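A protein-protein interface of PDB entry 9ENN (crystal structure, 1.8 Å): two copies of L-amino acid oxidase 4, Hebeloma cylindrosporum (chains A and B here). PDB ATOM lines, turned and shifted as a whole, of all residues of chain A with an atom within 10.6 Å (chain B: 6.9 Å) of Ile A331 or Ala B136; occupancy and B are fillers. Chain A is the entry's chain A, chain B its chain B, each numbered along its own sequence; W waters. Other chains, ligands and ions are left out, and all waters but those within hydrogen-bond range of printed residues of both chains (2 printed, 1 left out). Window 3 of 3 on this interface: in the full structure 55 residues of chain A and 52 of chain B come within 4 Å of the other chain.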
ATOM      1  N   ARG A 320      22.630 -21.932  17.165  1.00  0.00           N
ATOM      2  CA  ARG A 320      22.303 -20.551  17.511  1.00  0.00           C
ATOM      3  C   ARG A 320      21.561 -19.818  16.397  1.00  0.00           C
ATOM      4  O   ARG A 320      20.956 -18.771  16.663  1.00  0.00           O
ATOM      5  CB  ARG A 320      23.587 -19.797  17.886  1.00  0.00           C
ATOM      6  CG  ARG A 320      24.219 -20.231  19.220  1.00  0.00           C
ATOM      7  CD  ARG A 320      23.731 -19.367  20.380  1.00  0.00           C
ATOM      8  NE  ARG A 320      24.232 -18.004  20.254  1.00  0.00           N
ATOM      9  CZ  ARG A 320      23.715 -16.948  20.870  1.00  0.00           C
ATOM     10  NH1 ARG A 320      22.700 -17.064  21.712  1.00  0.00           N
ATOM     11  NH2 ARG A 320      24.235 -15.746  20.639  1.00  0.00           N
ATOM     12  N   SER A 327      11.895 -26.014  22.423  1.00  0.00           N
ATOM     13  CA  SER A 327      12.818 -27.047  22.889  1.00  0.00           C
ATOM     14  C   SER A 327      13.170 -26.883  24.365  1.00  0.00           C
ATOM     15  O   SER A 327      13.840 -27.750  24.932  1.00  0.00           O
ATOM     16  CB  SER A 327      14.105 -27.059  22.049  1.00  0.00           C
ATOM     17  OG  SER A 327      13.899 -27.750  20.825  1.00  0.00           O
ATOM     18  N   LYS A 328      12.744 -25.789  24.988  1.00  0.00           N
ATOM     19  CA  LYS A 328      12.812 -25.628  26.437  1.00  0.00           C
ATOM     20  C   LYS A 328      14.218 -25.880  26.981  1.00  0.00           C
ATOM     21  O   LYS A 328      14.398 -26.542  28.008  1.00  0.00           O
ATOM     22  CB  LYS A 328      11.798 -26.540  27.139  1.00  0.00           C
ATOM     23  CG  LYS A 328      10.368 -26.274  26.731  1.00  0.00           C
ATOM     24  CD  LYS A 328       9.372 -26.814  27.740  1.00  0.00           C
ATOM     25  CE  LYS A 328       9.459 -28.299  27.985  1.00  0.00           C
ATOM     26  NZ  LYS A 328       8.384 -28.687  28.959  1.00  0.00           N
ATOM     27  N   LEU A 329      15.229 -25.324  26.320  1.00  0.00           N
ATOM     28  CA  LEU A 329      16.576 -25.366  26.876  1.00  0.00           C
ATOM     29  C   LEU A 329      16.582 -24.668  28.232  1.00  0.00           C
ATOM     30  O   LEU A 329      15.879 -23.676  28.434  1.00  0.00           O
ATOM     31  CB  LEU A 329      17.572 -24.682  25.937  1.00  0.00           C
ATOM     32  CG  LEU A 329      18.189 -25.550  24.839  1.00  0.00           C
ATOM     33  CD1 LEU A 329      17.120 -25.988  23.844  1.00  0.00           C
ATOM     34  CD2 LEU A 329      19.343 -24.817  24.136  1.00  0.00           C
ATOM     35  N   ASP A 330      17.335 -25.208  29.189  1.00  0.00           N
ATOM     36  CA  ASP A 330      17.472 -24.450  30.426  1.00  0.00           C
ATOM     37  C   ASP A 330      18.507 -23.338  30.221  1.00  0.00           C
ATOM     38  O   ASP A 330      19.180 -23.259  29.190  1.00  0.00           O
ATOM     39  CB  ASP A 330      17.816 -25.353  31.618  1.00  0.00           C
ATOM     40  CG  ASP A 330      19.192 -25.968  31.535  1.00  0.00           C
ATOM     41  OD1 ASP A 330      20.165 -25.248  31.237  1.00  0.00           O
ATOM     42  OD2 ASP A 330      19.306 -27.179  31.821  1.00  0.00           O
ATOM     43  N   ILE A 331      18.605 -22.446  31.211  1.00  0.00           N
ATOM     44  CA  ILE A 331      19.394 -21.226  31.048  1.00  0.00           C
ATOM     45  C   ILE A 331      20.875 -21.538  30.883  1.00  0.00           C
ATOM     46  O   ILE A 331      21.604 -20.790  30.215  1.00  0.00           O
ATOM     47  CB  ILE A 331      19.131 -20.282  32.241  1.00  0.00           C
ATOM     48  CG1 ILE A 331      19.758 -18.904  32.016  1.00  0.00           C
ATOM     49  CG2 ILE A 331      19.651 -20.889  33.551  1.00  0.00           C
ATOM     50  CD1 ILE A 331      19.228 -17.849  32.967  1.00  0.00           C
ATOM     51  N   VAL A 332      21.350 -22.633  31.478  1.00  0.00           N
ATOM     52  CA  VAL A 332      22.754 -22.998  31.306  1.00  0.00           C
ATOM     53  C   VAL A 332      22.994 -23.510  29.893  1.00  0.00           C
ATOM     54  O   VAL A 332      23.966 -23.126  29.233  1.00  0.00           O
ATOM     55  CB  VAL A 332      23.195 -24.036  32.354  1.00  0.00           C
ATOM     56  CG1 VAL A 332      24.704 -24.316  32.210  1.00  0.00           C
ATOM     57  CG2 VAL A 332      22.868 -23.553  33.761  1.00  0.00           C
ATOM     58  N   GLN A 333      22.110 -24.388  29.412  1.00  0.00           N
ATOM     59  CA  GLN A 333      22.233 -24.913  28.057  1.00  0.00           C
ATOM     60  C   GLN A 333      22.235 -23.798  27.017  1.00  0.00           C
ATOM     61  O   GLN A 333      23.023 -23.833  26.067  1.00  0.00           O
ATOM     62  CB  GLN A 333      21.095 -25.891  27.773  1.00  0.00           C
ATOM     63  CG  GLN A 333      21.137 -27.149  28.605  1.00  0.00           C
ATOM     64  CD  GLN A 333      19.931 -28.037  28.373  1.00  0.00           C
ATOM     65  OE1 GLN A 333      18.792 -27.558  28.309  1.00  0.00           O
ATOM     66  NE2 GLN A 333      20.172 -29.341  28.246  1.00  0.00           N
ATOM     67  N   SER A 334      21.333 -22.819  27.149  1.00  0.00           N
ATOM     68  CA  SER A 334      21.280 -21.754  26.147  1.00  0.00           C
ATOM     69  C   SER A 334      22.516 -20.860  26.219  1.00  0.00           C
ATOM     70  O   SER A 334      22.987 -20.369  25.184  1.00  0.00           O
ATOM     71  CB  SER A 334      19.981 -20.950  26.285  1.00  0.00           C
ATOM     72  OG  SER A 334      19.804 -20.397  27.572  1.00  0.00           O
ATOM     73  N   ASN A 335      23.077 -20.662  27.418  1.00  0.00           N
ATOM     74  CA  ASN A 335      24.355 -19.965  27.533  1.00  0.00           C
ATOM     75  C   ASN A 335      25.476 -20.778  26.903  1.00  0.00           C
ATOM     76  O   ASN A 335      26.378 -20.227  26.263  1.00  0.00           O
ATOM     77  CB  ASN A 335      24.676 -19.692  29.000  1.00  0.00           C
ATOM     78  CG  ASN A 335      24.177 -18.347  29.463  1.00  0.00           C
ATOM     79  OD1 ASN A 335      24.935 -17.375  29.502  1.00  0.00           O
ATOM     80  ND2 ASN A 335      22.899 -18.277  29.819  1.00  0.00           N
ATOM     81  N   ALA A 336      25.444 -22.093  27.104  1.00  0.00           N
ATOM     82  CA  ALA A 336      26.475 -22.959  26.553  1.00  0.00           C
ATOM     83  C   ALA A 336      26.548 -22.870  25.036  1.00  0.00           C
ATOM     84  O   ALA A 336      27.644 -22.890  24.462  1.00  0.00           O
ATOM     85  CB  ALA A 336      26.205 -24.400  26.982  1.00  0.00           C
ATOM     86  N   LEU A 337      25.394 -22.832  24.363  1.00  0.00           N
ATOM     87  CA  LEU A 337      25.408 -22.749  22.908  1.00  0.00           C
ATOM     88  C   LEU A 337      26.187 -21.531  22.440  1.00  0.00           C
ATOM     89  O   LEU A 337      26.838 -21.561  21.388  1.00  0.00           O
ATOM     90  CB  LEU A 337      23.990 -22.688  22.349  1.00  0.00           C
ATOM     91  CG  LEU A 337      23.097 -23.916  22.504  1.00  0.00           C
ATOM     92  CD1 LEU A 337      21.786 -23.688  21.756  1.00  0.00           C
ATOM     93  CD2 LEU A 337      23.810 -25.176  22.025  1.00  0.00           C
ATOM     94  N   ARG A 338      26.085 -20.427  23.181  1.00  0.00           N
ATOM     95  CA  ARG A 338      26.750 -19.200  22.771  1.00  0.00           C
ATOM     96  C   ARG A 338      28.219 -19.189  23.168  1.00  0.00           C
ATOM     97  O   ARG A 338      29.077 -18.804  22.369  1.00  0.00           O
ATOM     98  CB  ARG A 338      26.045 -17.990  23.379  1.00  0.00           C
ATOM     99  CG  ARG A 338      26.746 -16.663  23.112  1.00  0.00           C
ATOM    100  CD  ARG A 338      25.941 -15.510  23.694  1.00  0.00           C
ATOM    101  NE  ARG A 338      25.785 -15.626  25.141  1.00  0.00           N
ATOM    102  CZ  ARG A 338      26.687 -15.231  26.030  1.00  0.00           C
ATOM    103  NH1 ARG A 338      27.832 -14.682  25.657  1.00  0.00           N
ATOM    104  NH2 ARG A 338      26.428 -15.378  27.325  1.00  0.00           N
ATOM    105  N   LYS A 339      28.519 -19.594  24.400  1.00  0.00           N
ATOM    106  CA  LYS A 339      29.826 -19.347  24.991  1.00  0.00           C
ATOM    107  C   LYS A 339      30.844 -20.434  24.682  1.00  0.00           C
ATOM    108  O   LYS A 339      32.031 -20.119  24.551  1.00  0.00           O
ATOM    109  CB  LYS A 339      29.677 -19.191  26.513  1.00  0.00           C
ATOM    110  CG  LYS A 339      30.987 -19.115  27.309  1.00  0.00           C
ATOM    111  CD  LYS A 339      31.823 -17.899  26.939  1.00  0.00           C
ATOM    112  CE  LYS A 339      33.222 -17.956  27.555  1.00  0.00           C
ATOM    113  NZ  LYS A 339      34.082 -18.974  26.888  1.00  0.00           N
ATOM    114  N   LEU A 340      30.433 -21.696  24.569  1.00  0.00           N
ATOM    115  CA  LEU A 340      31.397 -22.764  24.307  1.00  0.00           C
ATOM    116  C   LEU A 340      32.133 -22.481  22.998  1.00  0.00           C
ATOM    117  O   LEU A 340      31.524 -22.417  21.925  1.00  0.00           O
ATOM    118  CB  LEU A 340      30.691 -24.121  24.278  1.00  0.00           C
ATOM    119  CG  LEU A 340      30.195 -24.643  25.637  1.00  0.00           C
ATOM    120  CD1 LEU A 340      29.456 -25.987  25.461  1.00  0.00           C
ATOM    121  CD2 LEU A 340      31.321 -24.787  26.673  1.00  0.00           C
ATOM    122  N   ASP A 479      32.358 -25.299  33.461  1.00  0.00           N
ATOM    123  CA  ASP A 479      31.156 -24.517  33.726  1.00  0.00           C
ATOM    124  C   ASP A 479      29.963 -24.900  32.870  1.00  0.00           C
ATOM    125  O   ASP A 479      28.844 -24.992  33.387  1.00  0.00           O
ATOM    126  CB  ASP A 479      31.471 -23.026  33.505  1.00  0.00           C
ATOM    127  CG  ASP A 479      30.313 -22.102  33.876  1.00  0.00           C
ATOM    128  OD1 ASP A 479      29.683 -22.328  34.928  1.00  0.00           O
ATOM    129  OD2 ASP A 479      30.056 -21.127  33.129  1.00  0.00           O
ATOM    130  N   LEU A 480      30.170 -25.113  31.570  1.00  0.00           N
ATOM    131  CA  LEU A 480      29.078 -25.171  30.609  1.00  0.00           C
ATOM    132  C   LEU A 480      28.954 -26.491  29.863  1.00  0.00           C
ATOM    133  O   LEU A 480      27.858 -26.804  29.384  1.00  0.00           O
ATOM    134  CB  LEU A 480      29.240 -24.043  29.577  1.00  0.00           C
ATOM    135  CG  LEU A 480      29.105 -22.641  30.174  1.00  0.00           C
ATOM    136  CD1 LEU A 480      29.649 -21.595  29.220  1.00  0.00           C
ATOM    137  CD2 LEU A 480      27.652 -22.363  30.515  1.00  0.00           C
ATOM    138  N   THR A 482      28.841 -29.719  30.694  1.00  0.00           N
ATOM    139  CA  THR A 482      27.955 -30.792  31.134  1.00  0.00           C
ATOM    140  C   THR A 482      26.496 -30.477  30.825  1.00  0.00           C
ATOM    141  O   THR A 482      25.686 -31.397  30.659  1.00  0.00           O
ATOM    142  CB  THR A 482      28.124 -31.068  32.628  1.00  0.00           C
ATOM    143  OG1 THR A 482      27.806 -29.893  33.381  1.00  0.00           O
ATOM    144  CG2 THR A 482      29.534 -31.485  32.944  1.00  0.00           C
ATOM    145  N   SER A 483      26.146 -29.191  30.721  1.00  0.00           N
ATOM    146  CA  SER A 483      24.750 -28.836  30.497  1.00  0.00           C
ATOM    147  C   SER A 483      24.235 -29.409  29.183  1.00  0.00           C
ATOM    148  O   SER A 483      23.064 -29.792  29.090  1.00  0.00           O
ATOM    149  CB  SER A 483      24.582 -27.315  30.515  1.00  0.00           C
ATOM    150  OG  SER A 483      25.115 -26.701  29.350  1.00  0.00           O
ATOM    151  N   LEU A 484      25.093 -29.518  28.169  1.00  0.00           N
ATOM    152  CA  LEU A 484      24.641 -30.017  26.877  1.00  0.00           C
ATOM    153  C   LEU A 484      24.700 -31.534  26.791  1.00  0.00           C
ATOM    154  O   LEU A 484      24.207 -32.101  25.811  1.00  0.00           O
ATOM    155  CB  LEU A 484      25.449 -29.399  25.733  1.00  0.00           C
ATOM    156  CG  LEU A 484      25.199 -27.893  25.626  1.00  0.00           C
ATOM    157  CD1 LEU A 484      26.060 -27.255  24.566  1.00  0.00           C
ATOM    158  CD2 LEU A 484      23.722 -27.594  25.350  1.00  0.00           C
ATOM    159  N   ARG A 486      23.104 -33.121  29.102  1.00  0.00           N
ATOM    160  CA  ARG A 486      21.728 -33.385  29.495  1.00  0.00           C
ATOM    161  C   ARG A 486      20.822 -33.089  28.304  1.00  0.00           C
ATOM    162  O   ARG A 486      21.068 -32.127  27.567  1.00  0.00           O
ATOM    163  CB  ARG A 486      21.287 -32.497  30.650  1.00  0.00           C
ATOM    164  CG  ARG A 486      22.124 -32.527  31.900  1.00  0.00           C
ATOM    165  CD  ARG A 486      21.412 -31.762  33.018  1.00  0.00           C
ATOM    166  NE  ARG A 486      21.277 -30.331  32.756  1.00  0.00           N
ATOM    167  CZ  ARG A 486      22.168 -29.417  33.120  1.00  0.00           C
ATOM    168  NH1 ARG A 486      23.280 -29.753  33.752  1.00  0.00           N
ATOM    169  NH2 ARG A 486      21.924 -28.133  32.870  1.00  0.00           N
ATOM    170  N   PRO A 487      19.758 -33.856  28.100  1.00  0.00           N
ATOM    171  CA  PRO A 487      18.848 -33.563  26.987  1.00  0.00           C
ATOM    172  C   PRO A 487      18.050 -32.301  27.270  1.00  0.00           C
ATOM    173  O   PRO A 487      17.987 -31.818  28.402  1.00  0.00           O
ATOM    174  CB  PRO A 487      17.942 -34.800  26.935  1.00  0.00           C
ATOM    175  CG  PRO A 487      17.938 -35.308  28.361  1.00  0.00           C
ATOM    176  CD  PRO A 487      19.322 -35.018  28.900  1.00  0.00           C
ATOM    177  N   ALA A 488      17.430 -31.772  26.219  1.00  0.00           N
ATOM    178  CA  ALA A 488      16.428 -30.713  26.319  1.00  0.00           C
ATOM    179  C   ALA A 488      15.080 -31.258  25.823  1.00  0.00           C
ATOM    180  O   ALA A 488      14.924 -32.458  25.576  1.00  0.00           O
ATOM    181  CB  ALA A 488      16.886 -29.469  25.551  1.00  0.00           C
ATOM    182  N   PHE A 495      21.815 -33.495  22.317  1.00  0.00           N
ATOM    183  CA  PHE A 495      22.877 -32.732  21.668  1.00  0.00           C
ATOM    184  C   PHE A 495      24.060 -33.652  21.396  1.00  0.00           C
ATOM    185  O   PHE A 495      24.539 -34.342  22.302  1.00  0.00           O
ATOM    186  CB  PHE A 495      23.309 -31.541  22.534  1.00  0.00           C
ATOM    187  CG  PHE A 495      22.191 -30.579  22.828  1.00  0.00           C
ATOM    188  CD1 PHE A 495      21.732 -29.716  21.850  1.00  0.00           C
ATOM    189  CD2 PHE A 495      21.584 -30.552  24.075  1.00  0.00           C
ATOM    190  CE1 PHE A 495      20.681 -28.839  22.109  1.00  0.00           C
ATOM    191  CE2 PHE A 495      20.539 -29.674  24.340  1.00  0.00           C
ATOM    192  CZ  PHE A 495      20.088 -28.819  23.356  1.00  0.00           C
ATOM    193  N   PHE B 119      17.992 -10.802  27.446  1.00  0.00           N
ATOM    194  CA  PHE B 119      18.960 -11.805  27.875  1.00  0.00           C
ATOM    195  C   PHE B 119      18.219 -12.944  28.558  1.00  0.00           C
ATOM    196  O   PHE B 119      17.329 -12.699  29.376  1.00  0.00           O
ATOM    197  CB  PHE B 119      20.006 -11.223  28.847  1.00  0.00           C
ATOM    198  CG  PHE B 119      20.957 -10.239  28.217  1.00  0.00           C
ATOM    199  CD1 PHE B 119      20.585  -8.915  28.046  1.00  0.00           C
ATOM    200  CD2 PHE B 119      22.231 -10.634  27.807  1.00  0.00           C
ATOM    201  CE1 PHE B 119      21.462  -7.995  27.467  1.00  0.00           C
ATOM    202  CE2 PHE B 119      23.116  -9.723  27.220  1.00  0.00           C
ATOM    203  CZ  PHE B 119      22.730  -8.401  27.051  1.00  0.00           C
ATOM    204  N   ASN B 120      18.582 -14.180  28.219  1.00  0.00           N
ATOM    205  CA  ASN B 120      17.983 -15.362  28.832  1.00  0.00           C
ATOM    206  C   ASN B 120      16.465 -15.359  28.680  1.00  0.00           C
ATOM    207  O   ASN B 120      15.738 -15.830  29.560  1.00  0.00           O
ATOM    208  CB  ASN B 120      18.380 -15.478  30.307  1.00  0.00           C
ATOM    209  CG  ASN B 120      19.884 -15.507  30.504  1.00  0.00           C
ATOM    210  OD1 ASN B 120      20.605 -16.224  29.809  1.00  0.00           O
ATOM    211  ND2 ASN B 120      20.365 -14.733  31.463  1.00  0.00           N
ATOM    212  N   PHE B 132      17.313 -10.624  34.654  1.00  0.00           N
ATOM    213  CA  PHE B 132      17.403 -11.486  33.473  1.00  0.00           C
ATOM    214  C   PHE B 132      17.567 -12.953  33.857  1.00  0.00           C
ATOM    215  O   PHE B 132      18.347 -13.692  33.255  1.00  0.00           O
ATOM    216  CB  PHE B 132      18.549 -11.023  32.561  1.00  0.00           C
ATOM    217  CG  PHE B 132      18.419  -9.589  32.136  1.00  0.00           C
ATOM    218  CD1 PHE B 132      17.563  -9.231  31.111  1.00  0.00           C
ATOM    219  CD2 PHE B 132      19.112  -8.588  32.797  1.00  0.00           C
ATOM    220  CE1 PHE B 132      17.413  -7.909  30.739  1.00  0.00           C
ATOM    221  CE2 PHE B 132      18.964  -7.262  32.426  1.00  0.00           C
ATOM    222  CZ  PHE B 132      18.112  -6.923  31.397  1.00  0.00           C
ATOM    223  N   ASP B 133      16.816 -13.383  34.870  1.00  0.00           N
ATOM    224  CA  ASP B 133      16.803 -14.779  35.300  1.00  0.00           C
ATOM    225  C   ASP B 133      18.160 -15.243  35.828  1.00  0.00           C
ATOM    226  O   ASP B 133      18.426 -16.446  35.887  1.00  0.00           O
ATOM    227  CB  ASP B 133      16.351 -15.683  34.144  1.00  0.00           C
ATOM    228  CG  ASP B 133      15.553 -16.889  34.602  1.00  0.00           C
ATOM    229  OD1 ASP B 133      14.900 -16.831  35.670  1.00  0.00           O
ATOM    230  OD2 ASP B 133      15.585 -17.903  33.867  1.00  0.00           O
ATOM    231  N   ALA B 134      19.028 -14.323  36.244  1.00  0.00           N
ATOM    232  CA  ALA B 134      20.321 -14.741  36.770  1.00  0.00           C
ATOM    233  C   ALA B 134      20.225 -15.670  37.980  1.00  0.00           C
ATOM    234  O   ALA B 134      21.112 -16.531  38.118  1.00  0.00           O
ATOM    235  CB  ALA B 134      21.177 -13.508  37.107  1.00  0.00           C
ATOM    236  N   PRO B 135      19.225 -15.573  38.872  1.00  0.00           N
ATOM    237  CA  PRO B 135      19.160 -16.575  39.950  1.00  0.00           C
ATOM    238  C   PRO B 135      19.136 -17.999  39.423  1.00  0.00           C
ATOM    239  O   PRO B 135      19.777 -18.877  40.012  1.00  0.00           O
ATOM    240  CB  PRO B 135      17.863 -16.222  40.693  1.00  0.00           C
ATOM    241  CG  PRO B 135      17.708 -14.756  40.470  1.00  0.00           C
ATOM    242  CD  PRO B 135      18.187 -14.536  39.039  1.00  0.00           C
ATOM    243  N   ALA B 136      18.436 -18.253  38.310  1.00  0.00           N
ATOM    244  CA  ALA B 136      18.397 -19.602  37.750  1.00  0.00           C
ATOM    245  C   ALA B 136      19.747 -20.035  37.187  1.00  0.00           C
ATOM    246  O   ALA B 136      20.003 -21.235  37.071  1.00  0.00           O
ATOM    247  CB  ALA B 136      17.335 -19.701  36.653  1.00  0.00           C
ATOM    248  N   LEU B 137      20.597 -19.087  36.810  1.00  0.00           N
ATOM    249  CA  LEU B 137      21.966 -19.363  36.394  1.00  0.00           C
ATOM    250  C   LEU B 137      22.894 -19.591  37.576  1.00  0.00           C
ATOM    251  O   LEU B 137      24.064 -19.929  37.371  1.00  0.00           O
ATOM    252  CB  LEU B 137      22.439 -18.184  35.553  1.00  0.00           C
ATOM    253  CG  LEU B 137      23.586 -18.226  34.561  1.00  0.00           C
ATOM    254  CD1 LEU B 137      23.488 -19.367  33.609  1.00  0.00           C
ATOM    255  CD2 LEU B 137      23.550 -16.876  33.832  1.00  0.00           C
ATOM    256  N   GLY B 138      22.408 -19.419  38.797  1.00  0.00           N
ATOM    257  CA  GLY B 138      23.241 -19.604  39.961  1.00  0.00           C
ATOM    258  C   GLY B 138      23.993 -18.375  40.402  1.00  0.00           C
ATOM    259  O   GLY B 138      25.019 -18.504  41.080  1.00  0.00           O
ATOM    260  N   ILE B 139      23.544 -17.188  40.010  1.00  0.00           N
ATOM    261  CA  ILE B 139      24.133 -15.947  40.488  1.00  0.00           C
ATOM    262  C   ILE B 139      23.390 -15.562  41.761  1.00  0.00           C
ATOM    263  O   ILE B 139      22.171 -15.352  41.735  1.00  0.00           O
ATOM    264  CB  ILE B 139      24.042 -14.829  39.443  1.00  0.00           C
ATOM    265  CG1 ILE B 139      24.570 -15.275  38.079  1.00  0.00           C
ATOM    266  CG2 ILE B 139      24.813 -13.613  39.946  1.00  0.00           C
ATOM    267  CD1 ILE B 139      26.025 -15.672  38.060  1.00  0.00           C
ATOM    268  N   ILE B 144      23.829  -9.997  42.299  1.00  0.00           N
ATOM    269  CA  ILE B 144      22.853  -9.329  41.447  1.00  0.00           C
ATOM    270  C   ILE B 144      22.602  -7.910  41.944  1.00  0.00           C
ATOM    271  O   ILE B 144      22.457  -6.974  41.149  1.00  0.00           O
ATOM    272  CB  ILE B 144      21.550 -10.147  41.381  1.00  0.00           C
ATOM    273  CG1 ILE B 144      21.800 -11.491  40.692  1.00  0.00           C
ATOM    274  CG2 ILE B 144      20.460  -9.346  40.652  1.00  0.00           C
ATOM    275  CD1 ILE B 144      20.630 -12.464  40.808  1.00  0.00           C
ATOM    276  N   ARG B 210      31.268 -19.392  36.485  1.00  0.00           N
ATOM    277  CA  ARG B 210      29.872 -19.044  36.214  1.00  0.00           C
ATOM    278  C   ARG B 210      29.644 -17.550  36.413  1.00  0.00           C
ATOM    279  O   ARG B 210      29.023 -16.890  35.571  1.00  0.00           O
ATOM    280  CB  ARG B 210      28.939 -19.861  37.116  1.00  0.00           C
ATOM    281  CG  ARG B 210      27.430 -19.563  36.988  1.00  0.00           C
ATOM    282  CD  ARG B 210      26.875 -19.935  35.616  1.00  0.00           C
ATOM    283  NE  ARG B 210      27.163 -21.325  35.283  1.00  0.00           N
ATOM    284  CZ  ARG B 210      26.412 -22.364  35.625  1.00  0.00           C
ATOM    285  NH1 ARG B 210      25.290 -22.213  36.314  1.00  0.00           N
ATOM    286  NH2 ARG B 210      26.797 -23.589  35.276  1.00  0.00           N
HETATM  287  O   HOH W   1      20.256 -17.768  27.623  1.00  0.00           O
HETATM  288  O   HOH W   2      22.831 -14.781  28.607  1.00  0.00           O
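Water W1 lies within hydrogen-bond range of OG of Ser A334 (2.7 Å), OD1 of Asn B120 (2.7 Å) and ND2 of Asn A335 (3.5 Å).
Water W2 lies within hydrogen-bond range of OD1 of Asn B120 and OD1 of Asn A335.
No position is printed for both chains.
Printed residues of chain A that touch a printed residue of chain B: Ile A331, Val A332, Asn A335 and Asp A479.
Of chain B, only Asn B120 (3.5 Å), Asp B133 (3.3 Å), Ala B136 (3.6 Å) and Leu B137 (3.8 Å) come within 4 Å of Ile A331.
Of chain A, only Ile A331 comes within 4 Å of Ala B136.
Asp B133 touches one residue of chain A.
No residue of chain A comes within 4 Å of Ala B134.
No residue of chain A comes within 4 Å of Pro B135.
Printed residues of chain A within 4 Å of Arg B210: Val A332 (3.8 Å) and Asp A479 (2.7 Å).
Printed residues of chain B within 4 Å of Asn A335: Asn B120 (3.1 Å) and Leu B137 (3.99 Å).
Printed residues of chain A within 4 Å of Leu B137: Ile A331 and Asn A335.
Of the printed residues of chain B, Val A332 touches Arg B210.
Of the printed residues of chain B, Asp A479 touches Arg B210 (2.7 Å).
Phe B132 touches none of the printed residues of chain A.
The nearest residue of chain A that does not touch Ala B136 is Val A332 (5.0 Å).
CD1 of Ile A331 touches CG of Asn B120 (3.5 Å).
O of Asp B133 touches CD1 of Ile A331, at 3.3 Å.
Ile A331 touches Ala B136 (CG2 to O, 3.6 Å).
Leu B137 touches Ile A331.
NH1 of Arg B210 touches CG2 of Val A332, 3.8 Å away.
Leu B137 touches Asn A335.
The side-chain amide nitrogen of Asn B120 is in hydrogen-bond range of the backbone carbonyl oxygen of Phe B132 (2.9 Å).
The backbone carbonyl oxygen (O) of Ile A331 sits at hydrogen-bond distance from the side-chain hydroxyl (OG) of Ser A334.
The backbone carbonyl oxygen (O) of Ile A331 lies within hydrogen-bond range of the side-chain amide nitrogen (ND2) of Asn A335.
The backbone carbonyl oxygen (O) of Leu B137 is in hydrogen-bond range of the guanidinium group (NH1) of Arg B210.
The side-chain carboxylate of Asp A330 is in hydrogen-bond range of the backbone NH of Val A332, at 2.9 Å.
NH2 of Arg A338 is in hydrogen-bond range of OD1 of Asn A335 (3.3 Å).
OD1 of Asn B120 is in hydrogen-bond range of ND2 of Asn A335, 3.1 Å away.
NE of Arg B210 is in salt-bridge range of OD1 of Asp A479 (2.7 Å).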
